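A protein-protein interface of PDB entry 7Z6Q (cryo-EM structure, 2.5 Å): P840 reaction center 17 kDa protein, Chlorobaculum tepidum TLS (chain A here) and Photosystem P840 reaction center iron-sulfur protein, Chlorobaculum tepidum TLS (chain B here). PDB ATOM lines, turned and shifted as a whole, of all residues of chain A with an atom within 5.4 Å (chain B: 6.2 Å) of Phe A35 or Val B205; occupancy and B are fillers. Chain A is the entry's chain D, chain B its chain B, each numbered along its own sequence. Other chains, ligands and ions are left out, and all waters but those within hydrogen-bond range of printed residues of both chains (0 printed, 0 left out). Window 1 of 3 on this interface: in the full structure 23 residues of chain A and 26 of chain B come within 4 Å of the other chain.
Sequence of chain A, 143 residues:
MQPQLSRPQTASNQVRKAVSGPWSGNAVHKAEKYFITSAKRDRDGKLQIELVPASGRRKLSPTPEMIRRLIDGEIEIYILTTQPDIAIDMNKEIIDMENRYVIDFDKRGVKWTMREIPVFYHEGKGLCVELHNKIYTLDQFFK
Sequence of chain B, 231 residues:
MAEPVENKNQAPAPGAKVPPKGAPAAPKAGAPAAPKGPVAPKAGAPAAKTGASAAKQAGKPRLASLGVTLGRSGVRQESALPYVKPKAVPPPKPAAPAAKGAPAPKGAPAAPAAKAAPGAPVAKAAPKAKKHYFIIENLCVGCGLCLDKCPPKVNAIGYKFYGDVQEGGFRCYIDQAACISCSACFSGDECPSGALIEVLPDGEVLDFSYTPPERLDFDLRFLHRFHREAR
Along chain A the printed residues that touch a printed residue of chain B span positions 35 to 116. Among the printed residues, 11 pairs touch across the chains. Among the printed residues, no Asp or Glu carboxylate lies within 4 Å of a Lys or Arg side-chain nitrogen of the other chain.
Printed residues of chain B within 4 Å of Phe A35: Val B205 (3.8 Å). Val B205 touches just these residues of chain A: Phe A35, Val A52, Pro A53, Ala A54 and Leu A80. Of the printed residues of chain A, Gly B203 touches Thr A37. Printed residues of chain B within 4 Å of Ser A55: Leu B206 (3.6 Å). Printed residues of chain B within 4 Å of Thr A37: Gly B203 (3.2 Å). Tyr A34 touches none of the printed residues of chain B. Leu A51 touches none of the printed residues of chain B. The nearest residue of chain B that does not touch Phe A35 is Ile B136 (4.2 Å).
O of Glu B198 is in hydrogen-bond range of N of Leu B206 (2.8 Å). N of Ala A54 is in hydrogen-bond range of O of Lys A33, at 2.7 Å. The backbone NH (N) of Phe A35 lies within hydrogen-bond range of the backbone carbonyl oxygen (O) of Val A52 (2.8 Å). NZ of Lys A33 is in salt-bridge range of OE1 of Glu A116 (3.2 Å). N of Thr A37 sits at hydrogen-bond distance from O of Glu A50 (2.9 Å).
O of Ala A54 sits at hydrogen-bond distance from N of Asp B207. O of Ala A54 sits close to O of Val B205.
Phe A35 touches Val B205. Thr A37 touches Gly B203 (CB to O, 3.2 Å). Val B205 touches Val A52 (N to CG2, 3.9 Å). Val B205 touches Pro A53 (O to O, 3.6 Å). Ala A54 touches Leu B206 (O to CA, 3.5 Å). O of Ser A55 touches CG of Leu B206, at 3.6 Å. CD1 of Leu A80 touches CD1 of Ile B197, at 3.8 Å. Val B205 touches Leu A80. Glu A116 touches Ile B136.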
ATOM      1  N   LYS A  33      16.699  -9.661  17.744  1.00  0.00           N
ATOM      2  CA  LYS A  33      16.399 -10.488  16.588  1.00  0.00           C
ATOM      3  C   LYS A  33      16.476  -9.653  15.323  1.00  0.00           C
ATOM      4  O   LYS A  33      15.922  -8.551  15.271  1.00  0.00           O
ATOM      5  CB  LYS A  33      15.010 -11.095  16.732  1.00  0.00           C
ATOM      6  CG  LYS A  33      14.754 -12.318  15.909  1.00  0.00           C
ATOM      7  CD  LYS A  33      13.375 -12.813  16.248  1.00  0.00           C
ATOM      8  CE  LYS A  33      13.015 -14.045  15.478  1.00  0.00           C
ATOM      9  NZ  LYS A  33      11.649 -14.497  15.826  1.00  0.00           N
ATOM     10  N   TYR A  34      17.145 -10.182  14.302  1.00  0.00           N
ATOM     11  CA  TYR A  34      17.305  -9.486  13.035  1.00  0.00           C
ATOM     12  C   TYR A  34      16.916 -10.403  11.886  1.00  0.00           C
ATOM     13  O   TYR A  34      17.081 -11.623  11.956  1.00  0.00           O
ATOM     14  CB  TYR A  34      18.742  -8.992  12.840  1.00  0.00           C
ATOM     15  CG  TYR A  34      19.212  -8.005  13.884  1.00  0.00           C
ATOM     16  CD1 TYR A  34      19.547  -8.423  15.162  1.00  0.00           C
ATOM     17  CD2 TYR A  34      19.334  -6.654  13.587  1.00  0.00           C
ATOM     18  CE1 TYR A  34      19.979  -7.525  16.112  1.00  0.00           C
ATOM     19  CE2 TYR A  34      19.772  -5.753  14.532  1.00  0.00           C
ATOM     20  CZ  TYR A  34      20.092  -6.193  15.794  1.00  0.00           C
ATOM     21  OH  TYR A  34      20.525  -5.301  16.745  1.00  0.00           O
ATOM     22  N   PHE A  35      16.383  -9.825  10.834  1.00  0.00           N
ATOM     23  CA  PHE A  35      15.969 -10.598   9.656  1.00  0.00           C
ATOM     24  C   PHE A  35      16.648 -10.050   8.409  1.00  0.00           C
ATOM     25  O   PHE A  35      16.459  -8.905   8.108  1.00  0.00           O
ATOM     26  CB  PHE A  35      14.464 -10.456   9.448  1.00  0.00           C
ATOM     27  CG  PHE A  35      13.613 -11.191  10.455  1.00  0.00           C
ATOM     28  CD1 PHE A  35      13.615 -10.830  11.789  1.00  0.00           C
ATOM     29  CD2 PHE A  35      12.799 -12.243  10.074  1.00  0.00           C
ATOM     30  CE1 PHE A  35      12.856 -11.515  12.716  1.00  0.00           C
ATOM     31  CE2 PHE A  35      12.006 -12.895  11.003  1.00  0.00           C
ATOM     32  CZ  PHE A  35      12.045 -12.539  12.321  1.00  0.00           C
ATOM     33  N   ILE A  36      17.384 -10.896   7.691  1.00  0.00           N
ATOM     34  CA  ILE A  36      17.980 -10.533   6.411  1.00  0.00           C
ATOM     35  C   ILE A  36      16.851 -10.301   5.416  1.00  0.00           C
ATOM     36  O   ILE A  36      16.108 -11.226   5.070  1.00  0.00           O
ATOM     37  CB  ILE A  36      18.945 -11.620   5.926  1.00  0.00           C
ATOM     38  CG1 ILE A  36      20.160 -11.700   6.852  1.00  0.00           C
ATOM     39  CG2 ILE A  36      19.378 -11.353   4.496  1.00  0.00           C
ATOM     40  CD1 ILE A  36      20.861 -13.032   6.826  1.00  0.00           C
ATOM     41  N   THR A  37      16.709  -9.057   4.953  1.00  0.00           N
ATOM     42  CA  THR A  37      15.542  -8.681   4.168  1.00  0.00           C
ATOM     43  C   THR A  37      15.790  -8.604   2.668  1.00  0.00           C
ATOM     44  O   THR A  37      14.839  -8.765   1.898  1.00  0.00           O
ATOM     45  CB  THR A  37      14.986  -7.333   4.647  1.00  0.00           C
ATOM     46  OG1 THR A  37      16.002  -6.327   4.551  1.00  0.00           O
ATOM     47  CG2 THR A  37      14.519  -7.443   6.087  1.00  0.00           C
ATOM     48  N   GLU A  50      21.591  -6.924   3.851  1.00  0.00           N
ATOM     49  CA  GLU A  50      20.986  -5.971   4.772  1.00  0.00           C
ATOM     50  C   GLU A  50      20.048  -6.722   5.709  1.00  0.00           C
ATOM     51  O   GLU A  50      19.163  -7.462   5.259  1.00  0.00           O
ATOM     52  CB  GLU A  50      20.255  -4.847   4.035  1.00  0.00           C
ATOM     53  CG  GLU A  50      19.042  -5.256   3.227  1.00  0.00           C
ATOM     54  CD  GLU A  50      18.426  -4.085   2.487  1.00  0.00           C
ATOM     55  OE1 GLU A  50      18.967  -2.964   2.594  1.00  0.00           O
ATOM     56  OE2 GLU A  50      17.402  -4.284   1.803  1.00  0.00           O
ATOM     57  N   LEU A  51      20.268  -6.552   7.007  1.00  0.00           N
ATOM     58  CA  LEU A  51      19.429  -7.142   8.036  1.00  0.00           C
ATOM     59  C   LEU A  51      18.836  -6.027   8.882  1.00  0.00           C
ATOM     60  O   LEU A  51      19.546  -5.102   9.291  1.00  0.00           O
ATOM     61  CB  LEU A  51      20.225  -8.138   8.890  1.00  0.00           C
ATOM     62  CG  LEU A  51      21.536  -7.726   9.560  1.00  0.00           C
ATOM     63  CD1 LEU A  51      21.286  -7.081  10.901  1.00  0.00           C
ATOM     64  CD2 LEU A  51      22.439  -8.935   9.714  1.00  0.00           C
ATOM     65  N   VAL A  52      17.516  -6.063   9.023  1.00  0.00           N
ATOM     66  CA  VAL A  52      16.800  -5.063   9.856  1.00  0.00           C
ATOM     67  C   VAL A  52      16.380  -5.789  11.131  1.00  0.00           C
ATOM     68  O   VAL A  52      16.127  -6.997  11.061  1.00  0.00           O
ATOM     69  CB  VAL A  52      15.593  -4.483   9.098  1.00  0.00           C
ATOM     70  CG1 VAL A  52      15.997  -3.988   7.721  1.00  0.00           C
ATOM     71  CG2 VAL A  52      14.461  -5.489   8.991  1.00  0.00           C
ATOM     72  N   PRO A  53      16.237  -5.112  12.289  1.00  0.00           N
ATOM     73  CA  PRO A  53      15.829  -5.773  13.528  1.00  0.00           C
ATOM     74  C   PRO A  53      14.333  -6.129  13.526  1.00  0.00           C
ATOM     75  O   PRO A  53      13.593  -5.667  12.680  1.00  0.00           O
ATOM     76  CB  PRO A  53      16.150  -4.748  14.626  1.00  0.00           C
ATOM     77  CG  PRO A  53      16.950  -3.669  13.931  1.00  0.00           C
ATOM     78  CD  PRO A  53      16.492  -3.691  12.490  1.00  0.00           C
ATOM     79  N   ALA A  54      13.882  -6.899  14.521  1.00  0.00           N
ATOM     80  CA  ALA A  54      12.451  -7.291  14.580  1.00  0.00           C
ATOM     81  C   ALA A  54      11.565  -6.035  14.645  1.00  0.00           C
ATOM     82  O   ALA A  54      10.526  -6.032  13.966  1.00  0.00           O
ATOM     83  CB  ALA A  54      12.212  -8.222  15.738  1.00  0.00           C
ATOM     84  N   SER A  55      11.977  -5.003  15.396  1.00  0.00           N
ATOM     85  CA  SER A  55      11.257  -3.701  15.457  1.00  0.00           C
ATOM     86  C   SER A  55      11.209  -3.116  14.039  1.00  0.00           C
ATOM     87  O   SER A  55      10.146  -2.632  13.636  1.00  0.00           O
ATOM     88  CB  SER A  55      11.951  -2.753  16.403  1.00  0.00           C
ATOM     89  OG  SER A  55      11.916  -3.215  17.749  1.00  0.00           O
ATOM     90  N   GLY A  56      12.330  -3.175  13.314  1.00  0.00           N
ATOM     91  CA  GLY A  56      12.406  -2.786  11.892  1.00  0.00           C
ATOM     92  C   GLY A  56      12.439  -1.301  11.577  1.00  0.00           C
ATOM     93  O   GLY A  56      11.709  -0.906  10.654  1.00  0.00           O
ATOM     94  N   ILE A  77      20.064 -13.946  14.033  1.00  0.00           N
ATOM     95  CA  ILE A  77      19.727 -13.570  12.665  1.00  0.00           C
ATOM     96  C   ILE A  77      18.960 -14.710  12.016  1.00  0.00           C
ATOM     97  O   ILE A  77      19.261 -15.888  12.243  1.00  0.00           O
ATOM     98  CB  ILE A  77      20.980 -13.222  11.835  1.00  0.00           C
ATOM     99  CG1 ILE A  77      21.811 -12.154  12.541  1.00  0.00           C
ATOM    100  CG2 ILE A  77      20.589 -12.736  10.451  1.00  0.00           C
ATOM    101  CD1 ILE A  77      22.963 -12.713  13.332  1.00  0.00           C
ATOM    102  N   TYR A  78      17.964 -14.358  11.211  1.00  0.00           N
ATOM    103  CA  TYR A  78      17.103 -15.345  10.586  1.00  0.00           C
ATOM    104  C   TYR A  78      16.735 -14.905   9.178  1.00  0.00           C
ATOM    105  O   TYR A  78      16.780 -13.721   8.837  1.00  0.00           O
ATOM    106  CB  TYR A  78      15.833 -15.561  11.400  1.00  0.00           C
ATOM    107  CG  TYR A  78      16.035 -16.074  12.809  1.00  0.00           C
ATOM    108  CD1 TYR A  78      16.177 -15.196  13.874  1.00  0.00           C
ATOM    109  CD2 TYR A  78      16.034 -17.433  13.081  1.00  0.00           C
ATOM    110  CE1 TYR A  78      16.347 -15.657  15.163  1.00  0.00           C
ATOM    111  CE2 TYR A  78      16.201 -17.904  14.369  1.00  0.00           C
ATOM    112  CZ  TYR A  78      16.357 -17.012  15.406  1.00  0.00           C
ATOM    113  OH  TYR A  78      16.523 -17.477  16.689  1.00  0.00           O
ATOM    114  N   ILE A  79      16.308 -15.873   8.369  1.00  0.00           N
ATOM    115  CA  ILE A  79      15.884 -15.591   6.968  1.00  0.00           C
ATOM    116  C   ILE A  79      14.504 -16.217   6.758  1.00  0.00           C
ATOM    117  O   ILE A  79      14.292 -17.329   7.244  1.00  0.00           O
ATOM    118  CB  ILE A  79      16.907 -16.158   5.964  1.00  0.00           C
ATOM    119  CG1 ILE A  79      18.283 -15.503   6.109  1.00  0.00           C
ATOM    120  CG2 ILE A  79      16.382 -16.052   4.543  1.00  0.00           C
ATOM    121  CD1 ILE A  79      19.384 -16.194   5.338  1.00  0.00           C
ATOM    122  N   LEU A  80      13.584 -15.494   6.124  1.00  0.00           N
ATOM    123  CA  LEU A  80      12.253 -16.071   5.811  1.00  0.00           C
ATOM    124  C   LEU A  80      12.403 -16.918   4.545  1.00  0.00           C
ATOM    125  O   LEU A  80      13.274 -16.592   3.728  1.00  0.00           O
ATOM    126  CB  LEU A  80      11.229 -14.950   5.611  1.00  0.00           C
ATOM    127  CG  LEU A  80      11.169 -13.886   6.708  1.00  0.00           C
ATOM    128  CD1 LEU A  80       9.925 -13.034   6.548  1.00  0.00           C
ATOM    129  CD2 LEU A  80      11.208 -14.511   8.093  1.00  0.00           C
ATOM    130  N   GLU A 116      11.536 -19.753   9.557  1.00  0.00           N
ATOM    131  CA  GLU A 116      12.649 -18.813   9.837  1.00  0.00           C
ATOM    132  C   GLU A 116      13.912 -19.658  10.035  1.00  0.00           C
ATOM    133  O   GLU A 116      13.959 -20.415  11.016  1.00  0.00           O
ATOM    134  CB  GLU A 116      12.323 -17.918  11.038  1.00  0.00           C
ATOM    135  CG  GLU A 116      12.127 -18.673  12.343  1.00  0.00           C
ATOM    136  CD  GLU A 116      12.271 -17.838  13.606  1.00  0.00           C
ATOM    137  OE1 GLU A 116      12.216 -16.601  13.503  1.00  0.00           O
ATOM    138  OE2 GLU A 116      12.445 -18.424  14.687  1.00  0.00           O
ATOM    139  N   ILE B 136       5.104 -17.146  10.817  1.00  0.00           N
ATOM    140  CA  ILE B 136       6.325 -17.908  11.026  1.00  0.00           C
ATOM    141  C   ILE B 136       5.916 -19.224  11.684  1.00  0.00           C
ATOM    142  O   ILE B 136       5.584 -19.259  12.869  1.00  0.00           O
ATOM    143  CB  ILE B 136       7.343 -17.152  11.870  1.00  0.00           C
ATOM    144  CG1 ILE B 136       7.592 -15.751  11.327  1.00  0.00           C
ATOM    145  CG2 ILE B 136       8.590 -17.861  11.764  1.00  0.00           C
ATOM    146  CD1 ILE B 136       8.583 -14.971  12.155  1.00  0.00           C
ATOM    147  N   ILE B 197       3.895 -11.782  11.169  1.00  0.00           N
ATOM    148  CA  ILE B 197       4.844 -10.727  10.852  1.00  0.00           C
ATOM    149  C   ILE B 197       4.375 -10.015   9.596  1.00  0.00           C
ATOM    150  O   ILE B 197       3.569 -10.533   8.817  1.00  0.00           O
ATOM    151  CB  ILE B 197       6.277 -11.250  10.643  1.00  0.00           C
ATOM    152  CG1 ILE B 197       6.320 -12.163   9.419  1.00  0.00           C
ATOM    153  CG2 ILE B 197       6.782 -11.956  11.887  1.00  0.00           C
ATOM    154  CD1 ILE B 197       6.841 -11.490   8.197  1.00  0.00           C
ATOM    155  N   GLU B 198       4.905  -8.815   9.402  1.00  0.00           N
ATOM    156  CA  GLU B 198       4.506  -7.989   8.282  1.00  0.00           C
ATOM    157  C   GLU B 198       5.752  -7.570   7.517  1.00  0.00           C
ATOM    158  O   GLU B 198       6.774  -7.223   8.119  1.00  0.00           O
ATOM    159  CB  GLU B 198       3.756  -6.759   8.761  1.00  0.00           C
ATOM    160  CG  GLU B 198       3.498  -5.749   7.676  1.00  0.00           C
ATOM    161  CD  GLU B 198       3.073  -4.420   8.239  1.00  0.00           C
ATOM    162  OE1 GLU B 198       3.252  -4.203   9.443  1.00  0.00           O
ATOM    163  OE2 GLU B 198       2.386  -3.669   7.534  1.00  0.00           O
ATOM    164  N   VAL B 199       5.669  -7.612   6.193  1.00  0.00           N
ATOM    165  CA  VAL B 199       6.738  -7.171   5.311  1.00  0.00           C
ATOM    166  C   VAL B 199       6.231  -5.956   4.549  1.00  0.00           C
ATOM    167  O   VAL B 199       5.208  -6.029   3.851  1.00  0.00           O
ATOM    168  CB  VAL B 199       7.191  -8.286   4.354  1.00  0.00           C
ATOM    169  CG1 VAL B 199       8.445  -7.864   3.613  1.00  0.00           C
ATOM    170  CG2 VAL B 199       7.439  -9.573   5.126  1.00  0.00           C
ATOM    171  N   LEU B 200       6.947  -4.842   4.698  1.00  0.00           N
ATOM    172  CA  LEU B 200       6.587  -3.579   4.082  1.00  0.00           C
ATOM    173  C   LEU B 200       6.907  -3.626   2.586  1.00  0.00           C
ATOM    174  O   LEU B 200       7.620  -4.524   2.132  1.00  0.00           O
ATOM    175  CB  LEU B 200       7.342  -2.440   4.772  1.00  0.00           C
ATOM    176  CG  LEU B 200       6.728  -1.846   6.052  1.00  0.00           C
ATOM    177  CD1 LEU B 200       6.432  -2.927   7.064  1.00  0.00           C
ATOM    178  CD2 LEU B 200       7.577  -0.787   6.698  1.00  0.00           C
ATOM    179  N   GLY B 203      10.456  -4.021   2.187  1.00  0.00           N
ATOM    180  CA  GLY B 203      11.052  -5.269   2.623  1.00  0.00           C
ATOM    181  C   GLY B 203      11.367  -5.436   4.096  1.00  0.00           C
ATOM    182  O   GLY B 203      11.851  -6.507   4.476  1.00  0.00           O
ATOM    183  N   GLU B 204      11.123  -4.436   4.940  1.00  0.00           N
ATOM    184  CA  GLU B 204      11.394  -4.623   6.361  1.00  0.00           C
ATOM    185  C   GLU B 204      10.388  -5.589   6.978  1.00  0.00           C
ATOM    186  O   GLU B 204       9.213  -5.620   6.608  1.00  0.00           O
ATOM    187  CB  GLU B 204      11.358  -3.293   7.111  1.00  0.00           C
ATOM    188  CG  GLU B 204      12.210  -2.200   6.505  1.00  0.00           C
ATOM    189  CD  GLU B 204      11.427  -1.333   5.552  1.00  0.00           C
ATOM    190  OE1 GLU B 204      10.674  -1.897   4.733  1.00  0.00           O
ATOM    191  OE2 GLU B 204      11.543  -0.092   5.634  1.00  0.00           O
ATOM    192  N   VAL B 205      10.865  -6.379   7.935  1.00  0.00           N
ATOM    193  CA  VAL B 205      10.062  -7.403   8.592  1.00  0.00           C
ATOM    194  C   VAL B 205       9.743  -6.917   9.997  1.00  0.00           C
ATOM    195  O   VAL B 205      10.648  -6.712  10.817  1.00  0.00           O
ATOM    196  CB  VAL B 205      10.779  -8.759   8.621  1.00  0.00           C
ATOM    197  CG1 VAL B 205      10.079  -9.707   9.580  1.00  0.00           C
ATOM    198  CG2 VAL B 205      10.839  -9.352   7.224  1.00  0.00           C
ATOM    199  N   LEU B 206       8.456  -6.738  10.282  1.00  0.00           N
ATOM    200  CA  LEU B 206       7.987  -6.293  11.586  1.00  0.00           C
ATOM    201  C   LEU B 206       7.296  -7.451  12.291  1.00  0.00           C
ATOM    202  O   LEU B 206       6.320  -8.002  11.773  1.00  0.00           O
ATOM    203  CB  LEU B 206       7.024  -5.116  11.450  1.00  0.00           C
ATOM    204  CG  LEU B 206       7.577  -3.699  11.346  1.00  0.00           C
ATOM    205  CD1 LEU B 206       8.359  -3.492  10.063  1.00  0.00           C
ATOM    206  CD2 LEU B 206       6.424  -2.734  11.429  1.00  0.00           C
ATOM    207  N   ASP B 207       7.765  -7.771  13.497  1.00  0.00           N
ATOM    208  CA  ASP B 207       7.151  -8.874  14.281  1.00  0.00           C
ATOM    209  C   ASP B 207       6.020  -8.333  15.161  1.00  0.00           C
ATOM    210  O   ASP B 207       5.125  -9.118  15.494  1.00  0.00           O
ATOM    211  CB  ASP B 207       8.198  -9.620  15.106  1.00  0.00           C
ATOM    212  CG  ASP B 207       8.592  -8.894  16.375  1.00  0.00           C
ATOM    213  OD1 ASP B 207       8.564  -7.649  16.371  1.00  0.00           O
ATOM    214  OD2 ASP B 207       8.932  -9.578  17.347  1.00  0.00           O
